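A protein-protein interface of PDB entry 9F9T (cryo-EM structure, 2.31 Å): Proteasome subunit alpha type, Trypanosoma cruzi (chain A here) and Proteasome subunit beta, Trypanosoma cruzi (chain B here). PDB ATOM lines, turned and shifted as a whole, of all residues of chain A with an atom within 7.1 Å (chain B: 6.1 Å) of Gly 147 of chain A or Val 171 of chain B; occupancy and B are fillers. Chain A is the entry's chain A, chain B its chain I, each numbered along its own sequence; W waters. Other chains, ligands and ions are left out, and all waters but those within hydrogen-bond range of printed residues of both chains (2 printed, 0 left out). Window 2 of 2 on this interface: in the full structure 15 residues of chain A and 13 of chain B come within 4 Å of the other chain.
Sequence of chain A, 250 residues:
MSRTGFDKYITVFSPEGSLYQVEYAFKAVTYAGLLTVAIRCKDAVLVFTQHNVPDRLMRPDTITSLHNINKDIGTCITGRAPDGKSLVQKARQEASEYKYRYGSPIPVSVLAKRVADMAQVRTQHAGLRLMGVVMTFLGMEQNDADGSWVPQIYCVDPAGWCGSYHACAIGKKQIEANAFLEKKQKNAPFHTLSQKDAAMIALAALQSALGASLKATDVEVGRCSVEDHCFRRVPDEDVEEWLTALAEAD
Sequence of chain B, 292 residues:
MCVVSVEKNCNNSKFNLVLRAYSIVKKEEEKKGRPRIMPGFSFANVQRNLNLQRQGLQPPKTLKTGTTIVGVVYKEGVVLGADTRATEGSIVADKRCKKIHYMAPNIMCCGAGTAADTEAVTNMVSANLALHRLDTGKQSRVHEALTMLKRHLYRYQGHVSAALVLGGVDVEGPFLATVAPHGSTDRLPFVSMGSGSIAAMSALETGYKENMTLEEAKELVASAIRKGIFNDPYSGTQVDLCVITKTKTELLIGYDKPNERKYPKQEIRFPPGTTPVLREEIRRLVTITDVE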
ATOM      1  N   GLU A 141      -1.483   1.980 -26.221  1.00  0.00           N
ATOM      2  CA  GLU A 141      -2.365   0.856 -25.939  1.00  0.00           C
ATOM      3  C   GLU A 141      -2.250   0.477 -24.473  1.00  0.00           C
ATOM      4  O   GLU A 141      -1.161   0.469 -23.931  1.00  0.00           O
ATOM      5  CB  GLU A 141      -1.994  -0.322 -26.871  1.00  0.00           C
ATOM      6  CG  GLU A 141      -3.173  -1.229 -27.215  1.00  0.00           C
ATOM      7  CD  GLU A 141      -3.147  -1.917 -28.586  1.00  0.00           C
ATOM      8  OE1 GLU A 141      -2.695  -3.091 -28.668  1.00  0.00           O
ATOM      9  OE2 GLU A 141      -3.634  -1.329 -29.562  1.00  0.00           O
ATOM     10  N   GLN A 142      -3.372   0.190 -23.854  1.00  0.00           N
ATOM     11  CA  GLN A 142      -3.422  -0.208 -22.456  1.00  0.00           C
ATOM     12  C   GLN A 142      -3.185  -1.716 -22.312  1.00  0.00           C
ATOM     13  O   GLN A 142      -3.732  -2.497 -23.078  1.00  0.00           O
ATOM     14  CB  GLN A 142      -4.804   0.195 -21.980  1.00  0.00           C
ATOM     15  CG  GLN A 142      -4.993   0.067 -20.480  1.00  0.00           C
ATOM     16  CD  GLN A 142      -6.216   0.761 -19.902  1.00  0.00           C
ATOM     17  OE1 GLN A 142      -7.269   0.882 -20.523  1.00  0.00           O
ATOM     18  NE2 GLN A 142      -6.087   1.149 -18.648  1.00  0.00           N
ATOM     19  N   ASN A 143      -2.343  -2.131 -21.355  1.00  0.00           N
ATOM     20  CA  ASN A 143      -2.185  -3.526 -20.949  1.00  0.00           C
ATOM     21  C   ASN A 143      -3.292  -3.941 -19.975  1.00  0.00           C
ATOM     22  O   ASN A 143      -3.672  -3.165 -19.105  1.00  0.00           O
ATOM     23  CB  ASN A 143      -0.914  -3.781 -20.126  1.00  0.00           C
ATOM     24  CG  ASN A 143       0.373  -3.663 -20.911  1.00  0.00           C
ATOM     25  OD1 ASN A 143       0.495  -4.186 -22.021  1.00  0.00           O
ATOM     26  ND2 ASN A 143       1.351  -2.989 -20.319  1.00  0.00           N
ATOM     27  N   ASP A 144      -3.740  -5.208 -20.050  1.00  0.00           N
ATOM     28  CA  ASP A 144      -4.838  -5.685 -19.213  1.00  0.00           C
ATOM     29  C   ASP A 144      -4.426  -5.834 -17.743  1.00  0.00           C
ATOM     30  O   ASP A 144      -5.263  -5.703 -16.853  1.00  0.00           O
ATOM     31  CB  ASP A 144      -5.373  -7.034 -19.702  1.00  0.00           C
ATOM     32  CG  ASP A 144      -6.167  -7.017 -21.008  1.00  0.00           C
ATOM     33  OD1 ASP A 144      -7.025  -6.110 -21.184  1.00  0.00           O
ATOM     34  OD2 ASP A 144      -5.958  -7.970 -21.821  1.00  0.00           O
ATOM     35  N   ALA A 145      -3.138  -6.115 -17.503  1.00  0.00           N
ATOM     36  CA  ALA A 145      -2.650  -6.542 -16.200  1.00  0.00           C
ATOM     37  C   ALA A 145      -2.732  -5.400 -15.183  1.00  0.00           C
ATOM     38  O   ALA A 145      -3.516  -5.473 -14.241  1.00  0.00           O
ATOM     39  CB  ALA A 145      -1.240  -7.071 -16.344  1.00  0.00           C
ATOM     40  N   ASP A 146      -1.927  -4.347 -15.383  1.00  0.00           N
ATOM     41  CA  ASP A 146      -1.765  -3.266 -14.415  1.00  0.00           C
ATOM     42  C   ASP A 146      -2.440  -1.979 -14.882  1.00  0.00           C
ATOM     43  O   ASP A 146      -2.468  -0.987 -14.138  1.00  0.00           O
ATOM     44  CB  ASP A 146      -0.285  -2.956 -14.211  1.00  0.00           C
ATOM     45  CG  ASP A 146       0.494  -3.162 -15.496  1.00  0.00           C
ATOM     46  OD1 ASP A 146       0.493  -4.328 -15.974  1.00  0.00           O
ATOM     47  OD2 ASP A 146       1.046  -2.170 -16.024  1.00  0.00           O
ATOM     48  N   GLY A 147      -2.915  -1.986 -16.142  1.00  0.00           N
ATOM     49  CA  GLY A 147      -3.618  -0.848 -16.715  1.00  0.00           C
ATOM     50  C   GLY A 147      -2.690   0.272 -17.163  1.00  0.00           C
ATOM     51  O   GLY A 147      -3.180   1.375 -17.380  1.00  0.00           O
ATOM     52  N   SER A 148      -1.379  -0.026 -17.315  1.00  0.00           N
ATOM     53  CA  SER A 148      -0.427   0.925 -17.887  1.00  0.00           C
ATOM     54  C   SER A 148      -0.581   1.034 -19.414  1.00  0.00           C
ATOM     55  O   SER A 148      -1.041   0.114 -20.097  1.00  0.00           O
ATOM     56  CB  SER A 148       1.004   0.576 -17.553  1.00  0.00           C
ATOM     57  OG  SER A 148       1.556  -0.324 -18.512  1.00  0.00           O
ATOM     58  N   TRP A 149      -0.141   2.170 -19.938  1.00  0.00           N
ATOM     59  CA  TRP A 149      -0.284   2.519 -21.332  1.00  0.00           C
ATOM     60  C   TRP A 149       1.055   2.420 -22.031  1.00  0.00           C
ATOM     61  O   TRP A 149       2.006   3.011 -21.567  1.00  0.00           O
ATOM     62  CB  TRP A 149      -0.844   3.943 -21.462  1.00  0.00           C
ATOM     63  CG  TRP A 149      -2.286   4.062 -21.062  1.00  0.00           C
ATOM     64  CD1 TRP A 149      -2.787   4.257 -19.811  1.00  0.00           C
ATOM     65  CD2 TRP A 149      -3.433   3.956 -21.937  1.00  0.00           C
ATOM     66  NE1 TRP A 149      -4.163   4.279 -19.841  1.00  0.00           N
ATOM     67  CE2 TRP A 149      -4.588   4.104 -21.122  1.00  0.00           C
ATOM     68  CE3 TRP A 149      -3.596   3.728 -23.314  1.00  0.00           C
ATOM     69  CZ2 TRP A 149      -5.873   4.048 -21.649  1.00  0.00           C
ATOM     70  CZ3 TRP A 149      -4.872   3.645 -23.835  1.00  0.00           C
ATOM     71  CH2 TRP A 149      -5.990   3.823 -23.011  1.00  0.00           C
ATOM     72  N   GLN B 139      -8.688  -8.801 -22.899  1.00  0.00           N
ATOM     73  CA  GLN B 139      -9.791  -9.185 -22.026  1.00  0.00           C
ATOM     74  C   GLN B 139     -11.054  -8.387 -22.318  1.00  0.00           C
ATOM     75  O   GLN B 139     -10.996  -7.199 -22.603  1.00  0.00           O
ATOM     76  CB  GLN B 139      -9.372  -8.919 -20.599  1.00  0.00           C
ATOM     77  CG  GLN B 139     -10.419  -9.300 -19.576  1.00  0.00           C
ATOM     78  CD  GLN B 139      -9.899  -8.941 -18.200  1.00  0.00           C
ATOM     79  OE1 GLN B 139      -9.205  -7.931 -18.021  1.00  0.00           O
ATOM     80  NE2 GLN B 139     -10.207  -9.798 -17.234  1.00  0.00           N
ATOM     81  N   ARG B 141     -14.153  -6.088 -22.025  1.00  0.00           N
ATOM     82  CA  ARG B 141     -14.553  -5.034 -21.101  1.00  0.00           C
ATOM     83  C   ARG B 141     -16.044  -5.104 -20.811  1.00  0.00           C
ATOM     84  O   ARG B 141     -16.822  -5.410 -21.688  1.00  0.00           O
ATOM     85  CB  ARG B 141     -14.209  -3.679 -21.706  1.00  0.00           C
ATOM     86  CG  ARG B 141     -12.796  -3.555 -22.242  1.00  0.00           C
ATOM     87  CD  ARG B 141     -11.855  -3.124 -21.156  1.00  0.00           C
ATOM     88  NE  ARG B 141     -10.529  -2.784 -21.706  1.00  0.00           N
ATOM     89  CZ  ARG B 141      -9.908  -1.618 -21.534  1.00  0.00           C
ATOM     90  NH1 ARG B 141      -8.627  -1.526 -21.812  1.00  0.00           N
ATOM     91  NH2 ARG B 141     -10.528  -0.588 -20.969  1.00  0.00           N
ATOM     92  N   VAL B 169     -15.519  -7.604 -13.924  1.00  0.00           N
ATOM     93  CA  VAL B 169     -14.366  -6.856 -13.488  1.00  0.00           C
ATOM     94  C   VAL B 169     -13.365  -6.851 -14.612  1.00  0.00           C
ATOM     95  O   VAL B 169     -13.051  -7.906 -15.100  1.00  0.00           O
ATOM     96  CB  VAL B 169     -13.743  -7.454 -12.224  1.00  0.00           C
ATOM     97  CG1 VAL B 169     -12.628  -6.627 -11.656  1.00  0.00           C
ATOM     98  CG2 VAL B 169     -14.733  -7.624 -11.090  1.00  0.00           C
ATOM     99  N   ASP B 170     -12.852  -5.693 -14.981  1.00  0.00           N
ATOM    100  CA  ASP B 170     -11.892  -5.562 -16.047  1.00  0.00           C
ATOM    101  C   ASP B 170     -10.845  -4.557 -15.584  1.00  0.00           C
ATOM    102  O   ASP B 170     -10.889  -4.154 -14.429  1.00  0.00           O
ATOM    103  CB  ASP B 170     -12.561  -5.163 -17.366  1.00  0.00           C
ATOM    104  CG  ASP B 170     -13.216  -3.775 -17.390  1.00  0.00           C
ATOM    105  OD1 ASP B 170     -12.565  -2.805 -16.927  1.00  0.00           O
ATOM    106  OD2 ASP B 170     -14.387  -3.640 -17.878  1.00  0.00           O
ATOM    107  N   VAL B 171      -9.935  -4.124 -16.464  1.00  0.00           N
ATOM    108  CA  VAL B 171      -8.826  -3.289 -16.048  1.00  0.00           C
ATOM    109  C   VAL B 171      -9.288  -2.000 -15.363  1.00  0.00           C
ATOM    110  O   VAL B 171      -8.560  -1.485 -14.533  1.00  0.00           O
ATOM    111  CB  VAL B 171      -7.872  -2.995 -17.226  1.00  0.00           C
ATOM    112  CG1 VAL B 171      -8.474  -2.089 -18.290  1.00  0.00           C
ATOM    113  CG2 VAL B 171      -6.587  -2.402 -16.736  1.00  0.00           C
ATOM    114  N   GLU B 172     -10.503  -1.516 -15.619  1.00  0.00           N
ATOM    115  CA  GLU B 172     -10.975  -0.291 -14.987  1.00  0.00           C
ATOM    116  C   GLU B 172     -11.691  -0.544 -13.656  1.00  0.00           C
ATOM    117  O   GLU B 172     -12.344   0.341 -13.120  1.00  0.00           O
ATOM    118  CB  GLU B 172     -11.892   0.462 -15.959  1.00  0.00           C
ATOM    119  CG  GLU B 172     -11.147   0.936 -17.205  1.00  0.00           C
ATOM    120  CD  GLU B 172     -11.698   2.150 -17.939  1.00  0.00           C
ATOM    121  OE1 GLU B 172     -11.829   2.080 -19.195  1.00  0.00           O
ATOM    122  OE2 GLU B 172     -11.973   3.173 -17.265  1.00  0.00           O
ATOM    123  N   GLY B 173     -11.641  -1.772 -13.157  1.00  0.00           N
ATOM    124  CA  GLY B 173     -12.251  -2.120 -11.890  1.00  0.00           C
ATOM    125  C   GLY B 173     -13.590  -2.810 -12.046  1.00  0.00           C
ATOM    126  O   GLY B 173     -13.972  -3.225 -13.128  1.00  0.00           O
ATOM    127  N   LYS B 246     -10.859  -9.521  -9.755  1.00  0.00           N
ATOM    128  CA  LYS B 246      -9.923  -9.301 -10.843  1.00  0.00           C
ATOM    129  C   LYS B 246      -9.520 -10.647 -11.452  1.00  0.00           C
ATOM    130  O   LYS B 246      -9.401 -10.753 -12.677  1.00  0.00           O
ATOM    131  CB  LYS B 246      -8.659  -8.529 -10.438  1.00  0.00           C
ATOM    132  CG  LYS B 246      -7.965  -7.870 -11.632  1.00  0.00           C
ATOM    133  CD  LYS B 246      -6.877  -6.859 -11.262  1.00  0.00           C
ATOM    134  CE  LYS B 246      -5.735  -6.777 -12.282  1.00  0.00           C
ATOM    135  NZ  LYS B 246      -6.088  -6.089 -13.559  1.00  0.00           N
HETATM  136  O   HOH W   1      -9.147  -5.193 -22.145  1.00  0.00           O
HETATM  137  O   HOH W   2      -9.624  -5.498 -18.922  1.00  0.00           O
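Of the printed residues of chain B, Gln 142 of chain A touches Arg 141 (3.1 Å) and Val 171 (3.9 Å). Of the printed residues of chain B, Asn 143 of chain A touches Val 171 (3.8 Å). Of the printed residues of chain B, Asp 144 of chain A touches Gln 139, Val 171 and Lys 246. Gly 147 of chain A touches one residue of chain B. Printed residues of chain A within 4 Å of Arg 141 of chain B: Gln 142. Val 171 of chain B touches four residues of chain A. The nearest residue of chain A that does not touch Val 171 of chain B is Asp 146 of chain A (4.6 Å). The nearest printed residue of chain A that does not touch Gln 139 of chain B is Ala 145 of chain A (6.4 Å).
Of the 9 printed residues of chain A, 5 touch a printed residue of chain B. Printed residues of chain A that touch a printed residue of chain B: Gln 142, Asn 143, Asp 144, Ala 145 and Gly 147. Of the 8 printed residues of chain B, 4 touch a printed residue of chain A. Hydrophobic or aromatic side chains of chain B within 4 Å of the printed part of chain A: Val 171. Among the printed residues, no Asp or Glu carboxylate lies within 4 Å of a Lys or Arg side-chain nitrogen of the other chain.
Among the printed residues, pairs that only touch across the chains: Gln 142 of chain A with Val 171 of chain B, Asn 143 of chain A with Val 171 of chain B, Asp 144 of chain A with Val 171 of chain B and Gly 147 of chain A with Val 171 of chain B.
Water W1 lies within hydrogen-bond range of OD1 of Asp 144 of chain A (2.5 Å), O of Gln 139 of chain B (2.8 Å) and NE of Arg 141 of chain B (2.8 Å). Water W2 lies within hydrogen-bond range of OE1 of Gln 139 of chain B (2.6 Å), N of Val 171 of chain B (2.8 Å) and OD1 of Asp 144 of chain A (3.5 Å).
O of Asp 144 of chain A is in hydrogen-bond range of NZ of Lys 246 of chain B (3.4 Å). The side-chain amide oxygen (OE1) of Gln 142 of chain A is in hydrogen-bond range of the guanidinium group (NH1) of Arg 141 of chain B (3.1 Å). N of Gln 139 of chain B is in hydrogen-bond range of OD2 of Asp 144 of chain A (3.1 Å). The side-chain amino group of Lys 246 of chain B lies within hydrogen-bond range of the backbone carbonyl oxygen of Ala 145 of chain A, at 2.7 Å.
O of Gly 147 of chain A is in hydrogen-bond range of NE2 of Gln 142 of chain A (3.2 Å). The backbone NH (N) of Asn 143 of chain A is in hydrogen-bond range of the backbone carbonyl oxygen (O) of Ser 148 of chain A. The side-chain carboxylate (OE1) of Glu 172 of chain B is in salt-bridge range of the guanidinium group (NH2) of Arg 141 of chain B, at 3.5 Å.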
